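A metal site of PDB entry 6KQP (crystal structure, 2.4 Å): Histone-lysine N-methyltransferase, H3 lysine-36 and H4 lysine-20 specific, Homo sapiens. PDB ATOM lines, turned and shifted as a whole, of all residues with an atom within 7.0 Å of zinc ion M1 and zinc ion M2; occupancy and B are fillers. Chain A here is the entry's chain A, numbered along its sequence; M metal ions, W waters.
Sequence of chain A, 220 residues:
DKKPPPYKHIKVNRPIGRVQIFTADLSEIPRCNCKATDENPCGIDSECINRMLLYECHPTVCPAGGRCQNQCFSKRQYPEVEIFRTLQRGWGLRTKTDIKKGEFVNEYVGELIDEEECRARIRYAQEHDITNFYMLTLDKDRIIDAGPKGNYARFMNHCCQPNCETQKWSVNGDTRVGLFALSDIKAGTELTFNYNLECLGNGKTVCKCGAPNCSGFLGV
N of Cys 32 sits at hydrogen-bond distance from OD1 of Asn 50 (2.9 Å). The backbone carbonyl oxygen of Cys 42 sits at hydrogen-bond distance from the guanidinium group of Arg 51 (2.8 Å). The side-chain sulfur of Cys 68 sits close to the backbone NH of Asn 70 (3.4 Å). The side-chain hydroxyl (OG) of Ser 46 lies within hydrogen-bond range of the backbone NH (N) of Cys 48 (3.2 Å). The side-chain sulfur (SG) of Cys 48 sits close to the backbone NH (N) of Asn 50, at 3.7 Å. SG of Cys 48 sits close to N of Arg 51 (3.5 Å). The side-chain sulfur (SG) of Cys 62 sits close to the backbone NH (N) of Ala 64 (3.7 Å). O of Asn 70 lies within hydrogen-bond range of N of Cys 57, at 3.0 Å.
The nearest printed residue that does not touch zinc ion M1 is Cys 62 (4.4 Å).
Of the 27 residues printed, 4 come within 4 Å of zinc ion M2. The nearest printed residue that does not touch zinc ion M2 is Asn 70 (4.2 Å).
Zinc ion M1 is bound by SG of Cys 32 (2.1 Å), SG of Cys 48 (2.3 Å), SG of Cys 42 (2.3 Å) and SG of Cys 34 (2.4 Å).
Zinc ion M2 is bound by SG of Cys 42, at 2.1 Å. Zinc ion M2 is bound by SG of Cys 68 (2.2 Å). SG of Cys 62 binds zinc ion M2, at 2.4 Å. SG of Cys 57 binds zinc ion M2 (2.4 Å). Zinc ion M2 has four donor atoms within binding distance.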
ATOM      1  N   ARG A  31       7.979  12.625  28.732  1.00  0.00           N
ATOM      2  CA  ARG A  31       9.282  11.929  28.685  1.00  0.00           C
ATOM      3  C   ARG A  31      10.115  12.501  27.537  1.00  0.00           C
ATOM      4  O   ARG A  31       9.606  12.588  26.438  1.00  0.00           O
ATOM      5  CB  ARG A  31       9.049  10.443  28.476  1.00  0.00           C
ATOM      6  CG  ARG A  31       8.701   9.724  29.770  1.00  0.00           C
ATOM      7  CD  ARG A  31       8.028   8.412  29.429  1.00  0.00           C
ATOM      8  NE  ARG A  31       7.830   7.588  30.607  1.00  0.00           N
ATOM      9  CZ  ARG A  31       6.750   7.608  31.349  1.00  0.00           C
ATOM     10  NH1 ARG A  31       5.754   8.424  31.038  1.00  0.00           N
ATOM     11  NH2 ARG A  31       6.643   6.809  32.392  1.00  0.00           N
ATOM     12  N   CYS A  32      11.352  12.865  27.809  1.00  0.00           N
ATOM     13  CA  CYS A  32      12.234  13.433  26.772  1.00  0.00           C
ATOM     14  C   CYS A  32      12.938  12.337  25.959  1.00  0.00           C
ATOM     15  O   CYS A  32      12.805  11.170  26.285  1.00  0.00           O
ATOM     16  CB  CYS A  32      13.170  14.475  27.332  1.00  0.00           C
ATOM     17  SG  CYS A  32      14.757  13.869  27.913  1.00  0.00           S
ATOM     18  N   ASN A  33      13.587  12.744  24.880  1.00  0.00           N
ATOM     19  CA  ASN A  33      14.319  11.776  24.031  1.00  0.00           C
ATOM     20  C   ASN A  33      15.818  12.082  24.023  1.00  0.00           C
ATOM     21  O   ASN A  33      16.477  11.610  23.120  1.00  0.00           O
ATOM     22  CB  ASN A  33      13.728  11.678  22.625  1.00  0.00           C
ATOM     23  CG  ASN A  33      14.151  10.402  21.928  1.00  0.00           C
ATOM     24  OD1 ASN A  33      14.149   9.346  22.526  1.00  0.00           O
ATOM     25  ND2 ASN A  33      14.520  10.508  20.666  1.00  0.00           N
ATOM     26  N   CYS A  34      16.370  12.662  25.092  1.00  0.00           N
ATOM     27  CA  CYS A  34      17.837  12.844  25.195  1.00  0.00           C
ATOM     28  C   CYS A  34      18.498  11.475  25.429  1.00  0.00           C
ATOM     29  O   CYS A  34      17.817  10.493  25.839  1.00  0.00           O
ATOM     30  CB  CYS A  34      18.174  13.839  26.291  1.00  0.00           C
ATOM     31  SG  CYS A  34      17.317  15.436  26.124  1.00  0.00           S
ATOM     32  N   LYS A  35      19.791  11.391  25.190  1.00  0.00           N
ATOM     33  CA  LYS A  35      20.557  10.147  25.465  1.00  0.00           C
ATOM     34  C   LYS A  35      21.648  10.474  26.498  1.00  0.00           C
ATOM     35  O   LYS A  35      22.206  11.571  26.436  1.00  0.00           O
ATOM     36  CB  LYS A  35      21.109   9.567  24.150  1.00  0.00           C
ATOM     37  CG  LYS A  35      20.040   9.222  23.136  1.00  0.00           C
ATOM     38  CD  LYS A  35      20.495   9.172  21.701  1.00  0.00           C
ATOM     39  CE  LYS A  35      19.353   8.788  20.764  1.00  0.00           C
ATOM     40  NZ  LYS A  35      19.772   7.830  19.719  1.00  0.00           N
ATOM     41  N   ASP A  38      24.619  12.151  25.118  1.00  0.00           N
ATOM     42  CA  ASP A  38      24.573  13.549  24.580  1.00  0.00           C
ATOM     43  C   ASP A  38      25.611  14.366  25.370  1.00  0.00           C
ATOM     44  O   ASP A  38      25.995  13.928  26.471  1.00  0.00           O
ATOM     45  CB  ASP A  38      23.200  14.221  24.678  1.00  0.00           C
ATOM     46  CG  ASP A  38      22.076  13.533  23.901  1.00  0.00           C
ATOM     47  OD1 ASP A  38      22.394  12.708  23.016  1.00  0.00           O
ATOM     48  OD2 ASP A  38      20.885  13.806  24.199  1.00  0.00           O
ATOM     49  N   PRO A  41      23.327  16.179  28.591  1.00  0.00           N
ATOM     50  CA  PRO A  41      21.993  15.576  28.483  1.00  0.00           C
ATOM     51  C   PRO A  41      20.953  16.433  29.215  1.00  0.00           C
ATOM     52  O   PRO A  41      21.201  16.770  30.358  1.00  0.00           O
ATOM     53  CB  PRO A  41      22.169  14.195  29.146  1.00  0.00           C
ATOM     54  CG  PRO A  41      23.654  13.905  29.045  1.00  0.00           C
ATOM     55  CD  PRO A  41      24.321  15.266  29.164  1.00  0.00           C
ATOM     56  N   CYS A  42      19.862  16.787  28.532  1.00  0.00           N
ATOM     57  CA  CYS A  42      18.753  17.617  29.070  1.00  0.00           C
ATOM     58  C   CYS A  42      19.251  19.008  29.494  1.00  0.00           C
ATOM     59  O   CYS A  42      18.543  19.714  30.188  1.00  0.00           O
ATOM     60  CB  CYS A  42      18.076  16.884  30.220  1.00  0.00           C
ATOM     61  SG  CYS A  42      17.523  15.201  29.778  1.00  0.00           S
ATOM     62  N   GLY A  43      20.449  19.408  29.077  1.00  0.00           N
ATOM     63  CA  GLY A  43      21.050  20.682  29.495  1.00  0.00           C
ATOM     64  C   GLY A  43      20.431  21.848  28.761  1.00  0.00           C
ATOM     65  O   GLY A  43      19.602  21.615  27.861  1.00  0.00           O
ATOM     66  N   SER A  46      20.395  21.850  24.998  1.00  0.00           N
ATOM     67  CA  SER A  46      19.905  20.591  24.395  1.00  0.00           C
ATOM     68  C   SER A  46      18.551  20.847  23.721  1.00  0.00           C
ATOM     69  O   SER A  46      18.018  21.939  23.907  1.00  0.00           O
ATOM     70  CB  SER A  46      19.784  19.487  25.426  1.00  0.00           C
ATOM     71  OG  SER A  46      18.622  19.662  26.213  1.00  0.00           O
ATOM     72  N   GLU A  47      18.006  19.834  23.064  1.00  0.00           N
ATOM     73  CA  GLU A  47      16.655  19.862  22.434  1.00  0.00           C
ATOM     74  C   GLU A  47      15.670  19.105  23.327  1.00  0.00           C
ATOM     75  O   GLU A  47      14.654  18.628  22.804  1.00  0.00           O
ATOM     76  CB  GLU A  47      16.703  19.234  21.037  1.00  0.00           C
ATOM     77  CG  GLU A  47      17.869  19.697  20.166  1.00  0.00           C
ATOM     78  CD  GLU A  47      17.537  20.613  18.990  1.00  0.00           C
ATOM     79  OE1 GLU A  47      18.475  20.982  18.244  1.00  0.00           O
ATOM     80  OE2 GLU A  47      16.335  20.943  18.795  1.00  0.00           O
ATOM     81  N   CYS A  48      15.966  18.961  24.623  1.00  0.00           N
ATOM     82  CA  CYS A  48      15.104  18.249  25.599  1.00  0.00           C
ATOM     83  C   CYS A  48      13.658  18.767  25.486  1.00  0.00           C
ATOM     84  O   CYS A  48      13.435  19.979  25.667  1.00  0.00           O
ATOM     85  CB  CYS A  48      15.630  18.426  27.015  1.00  0.00           C
ATOM     86  SG  CYS A  48      14.691  17.485  28.248  1.00  0.00           S
ATOM     87  N   ILE A  49      12.718  17.884  25.153  1.00  0.00           N
ATOM     88  CA  ILE A  49      11.308  18.295  24.964  1.00  0.00           C
ATOM     89  C   ILE A  49      10.787  18.785  26.314  1.00  0.00           C
ATOM     90  O   ILE A  49      10.135  19.849  26.336  1.00  0.00           O
ATOM     91  CB  ILE A  49      10.443  17.168  24.342  1.00  0.00           C
ATOM     92  CG1 ILE A  49       9.004  17.649  24.071  1.00  0.00           C
ATOM     93  CG2 ILE A  49      10.428  15.903  25.169  1.00  0.00           C
ATOM     94  CD1 ILE A  49       8.918  18.869  23.161  1.00  0.00           C
ATOM     95  N   ASN A  50      11.093  18.063  27.414  1.00  0.00           N
ATOM     96  CA  ASN A  50      10.693  18.454  28.784  1.00  0.00           C
ATOM     97  C   ASN A  50      11.173  19.885  29.032  1.00  0.00           C
ATOM     98  O   ASN A  50      10.350  20.746  29.427  1.00  0.00           O
ATOM     99  CB  ASN A  50      11.249  17.510  29.828  1.00  0.00           C
ATOM    100  CG  ASN A  50      10.615  16.133  29.748  1.00  0.00           C
ATOM    101  OD1 ASN A  50      10.552  15.560  28.680  1.00  0.00           O
ATOM    102  ND2 ASN A  50      10.070  15.637  30.833  1.00  0.00           N
ATOM    103  N   ARG A  51      12.445  20.155  28.763  1.00  0.00           N
ATOM    104  CA  ARG A  51      13.029  21.500  29.026  1.00  0.00           C
ATOM    105  C   ARG A  51      12.265  22.537  28.197  1.00  0.00           C
ATOM    106  O   ARG A  51      11.958  23.614  28.729  1.00  0.00           O
ATOM    107  CB  ARG A  51      14.533  21.494  28.730  1.00  0.00           C
ATOM    108  CG  ARG A  51      15.213  22.774  29.192  1.00  0.00           C
ATOM    109  CD  ARG A  51      16.693  22.766  28.950  1.00  0.00           C
ATOM    110  NE  ARG A  51      17.463  22.339  30.123  1.00  0.00           N
ATOM    111  CZ  ARG A  51      17.717  23.082  31.185  1.00  0.00           C
ATOM    112  NH1 ARG A  51      17.209  24.299  31.303  1.00  0.00           N
ATOM    113  NH2 ARG A  51      18.444  22.590  32.156  1.00  0.00           N
ATOM    114  N   GLU A  56      10.379  19.700  34.297  1.00  0.00           N
ATOM    115  CA  GLU A  56      11.545  18.908  34.733  1.00  0.00           C
ATOM    116  C   GLU A  56      11.440  17.510  34.120  1.00  0.00           C
ATOM    117  O   GLU A  56      10.309  17.030  33.873  1.00  0.00           O
ATOM    118  CB  GLU A  56      11.608  18.793  36.258  1.00  0.00           C
ATOM    119  CG  GLU A  56      12.227  19.998  36.928  1.00  0.00           C
ATOM    120  CD  GLU A  56      12.670  19.756  38.363  1.00  0.00           C
ATOM    121  OE1 GLU A  56      12.463  18.618  38.879  1.00  0.00           O
ATOM    122  OE2 GLU A  56      13.242  20.689  38.965  1.00  0.00           O
ATOM    123  N   CYS A  57      12.578  16.895  33.822  1.00  0.00           N
ATOM    124  CA  CYS A  57      12.681  15.446  33.545  1.00  0.00           C
ATOM    125  C   CYS A  57      12.413  14.826  34.933  1.00  0.00           C
ATOM    126  O   CYS A  57      12.887  15.392  35.940  1.00  0.00           O
ATOM    127  CB  CYS A  57      14.039  15.087  32.920  1.00  0.00           C
ATOM    128  SG  CYS A  57      14.337  15.490  31.157  1.00  0.00           S
ATOM    129  N   HIS A  58      11.600  13.779  35.042  1.00  0.00           N
ATOM    130  CA  HIS A  58      11.507  12.989  36.296  1.00  0.00           C
ATOM    131  C   HIS A  58      12.650  11.973  36.345  1.00  0.00           C
ATOM    132  O   HIS A  58      12.900  11.258  35.373  1.00  0.00           O
ATOM    133  CB  HIS A  58      10.150  12.314  36.449  1.00  0.00           C
ATOM    134  CG  HIS A  58       9.958  11.798  37.831  1.00  0.00           C
ATOM    135  ND1 HIS A  58      10.510  10.614  38.248  1.00  0.00           N
ATOM    136  CD2 HIS A  58       9.361  12.335  38.915  1.00  0.00           C
ATOM    137  CE1 HIS A  58      10.223  10.422  39.524  1.00  0.00           C
ATOM    138  NE2 HIS A  58       9.512  11.466  39.949  1.00  0.00           N
ATOM    139  N   CYS A  62      13.867   9.505  33.128  1.00  0.00           N
ATOM    140  CA  CYS A  62      14.612  10.266  32.087  1.00  0.00           C
ATOM    141  C   CYS A  62      15.614   9.322  31.451  1.00  0.00           C
ATOM    142  O   CYS A  62      16.464   8.757  32.122  1.00  0.00           O
ATOM    143  CB  CYS A  62      15.299  11.516  32.582  1.00  0.00           C
ATOM    144  SG  CYS A  62      15.964  12.495  31.208  1.00  0.00           S
ATOM    145  N   PRO A  63      15.544   9.125  30.121  1.00  0.00           N
ATOM    146  CA  PRO A  63      16.473   8.214  29.448  1.00  0.00           C
ATOM    147  C   PRO A  63      17.955   8.605  29.675  1.00  0.00           C
ATOM    148  O   PRO A  63      18.800   7.764  29.423  1.00  0.00           O
ATOM    149  CB  PRO A  63      16.047   8.270  27.967  1.00  0.00           C
ATOM    150  CG  PRO A  63      15.267   9.564  27.833  1.00  0.00           C
ATOM    151  CD  PRO A  63      14.602   9.774  29.179  1.00  0.00           C
ATOM    152  N   ALA A  64      18.263   9.802  30.189  1.00  0.00           N
ATOM    153  CA  ALA A  64      19.653  10.261  30.430  1.00  0.00           C
ATOM    154  C   ALA A  64      20.129   9.936  31.855  1.00  0.00           C
ATOM    155  O   ALA A  64      21.279  10.335  32.229  1.00  0.00           O
ATOM    156  CB  ALA A  64      19.767  11.735  30.189  1.00  0.00           C
ATOM    157  N   GLY A  65      19.269   9.295  32.654  1.00  0.00           N
ATOM    158  CA  GLY A  65      19.640   8.803  33.989  1.00  0.00           C
ATOM    159  C   GLY A  65      20.233   9.900  34.861  1.00  0.00           C
ATOM    160  O   GLY A  65      19.680  11.053  34.841  1.00  0.00           O
ATOM    161  N   ARG A  67      22.814  11.639  34.540  1.00  0.00           N
ATOM    162  CA  ARG A  67      23.457  12.763  33.796  1.00  0.00           C
ATOM    163  C   ARG A  67      22.428  13.860  33.462  1.00  0.00           C
ATOM    164  O   ARG A  67      22.851  14.936  32.976  1.00  0.00           O
ATOM    165  CB  ARG A  67      24.147  12.240  32.549  1.00  0.00           C
ATOM    166  CG  ARG A  67      25.276  11.292  32.872  1.00  0.00           C
ATOM    167  CD  ARG A  67      26.008  10.900  31.608  1.00  0.00           C
ATOM    168  NE  ARG A  67      27.006   9.889  31.898  1.00  0.00           N
ATOM    169  CZ  ARG A  67      27.884   9.425  31.020  1.00  0.00           C
ATOM    170  NH1 ARG A  67      27.906   9.894  29.780  1.00  0.00           N
ATOM    171  NH2 ARG A  67      28.757   8.500  31.380  1.00  0.00           N
ATOM    172  N   CYS A  68      21.145  13.604  33.692  1.00  0.00           N
ATOM    173  CA  CYS A  68      20.065  14.563  33.367  1.00  0.00           C
ATOM    174  C   CYS A  68      20.363  15.911  34.038  1.00  0.00           C
ATOM    175  O   CYS A  68      20.588  15.930  35.237  1.00  0.00           O
ATOM    176  CB  CYS A  68      18.713  13.984  33.784  1.00  0.00           C
ATOM    177  SG  CYS A  68      17.345  15.150  33.671  1.00  0.00           S
ATOM    178  N   GLN A  69      20.387  16.992  33.270  1.00  0.00           N
ATOM    179  CA  GLN A  69      20.603  18.372  33.765  1.00  0.00           C
ATOM    180  C   GLN A  69      19.274  19.145  33.857  1.00  0.00           C
ATOM    181  O   GLN A  69      19.336  20.356  33.962  1.00  0.00           O
ATOM    182  CB  GLN A  69      21.588  19.066  32.832  1.00  0.00           C
ATOM    183  CG  GLN A  69      22.974  18.463  32.890  1.00  0.00           C
ATOM    184  CD  GLN A  69      23.902  19.156  31.935  1.00  0.00           C
ATOM    185  OE1 GLN A  69      23.627  20.260  31.460  1.00  0.00           O
ATOM    186  NE2 GLN A  69      25.003  18.487  31.603  1.00  0.00           N
ATOM    187  N   ASN A  70      18.133  18.466  33.890  1.00  0.00           N
ATOM    188  CA  ASN A  70      16.801  19.134  33.872  1.00  0.00           C
ATOM    189  C   ASN A  70      16.050  18.769  35.147  1.00  0.00           C
ATOM    190  O   ASN A  70      14.926  18.262  35.029  1.00  0.00           O
ATOM    191  CB  ASN A  70      15.985  18.739  32.638  1.00  0.00           C
ATOM    192  CG  ASN A  70      14.764  19.624  32.412  1.00  0.00           C
ATOM    193  OD1 ASN A  70      14.757  20.783  32.824  1.00  0.00           O
ATOM    194  ND2 ASN A  70      13.768  19.099  31.716  1.00  0.00           N
ATOM    195  N   GLN A  71      16.682  18.953  36.306  1.00  0.00           N
ATOM    196  CA  GLN A  71      16.030  18.759  37.625  1.00  0.00           C
ATOM    197  C   GLN A  71      16.372  19.923  38.550  1.00  0.00           C
ATOM    198  O   GLN A  71      16.448  19.684  39.780  1.00  0.00           O
ATOM    199  CB  GLN A  71      16.440  17.423  38.215  1.00  0.00           C
ATOM    200  CG  GLN A  71      15.818  16.240  37.514  1.00  0.00           C
ATOM    201  CD  GLN A  71      16.531  14.968  37.873  1.00  0.00           C
ATOM    202  OE1 GLN A  71      16.664  14.656  39.058  1.00  0.00           O
ATOM    203  NE2 GLN A  71      16.997  14.247  36.868  1.00  0.00           N
HETATM  204 ZN    ZN M   1      15.996  15.598  28.069  1.00  0.00          ZN
HETATM  205 ZN    ZN M   2      16.538  14.743  31.627  1.00  0.00          ZN
HETATM  206  O   HOH W   1      13.809  13.235  30.399  1.00  0.00           O
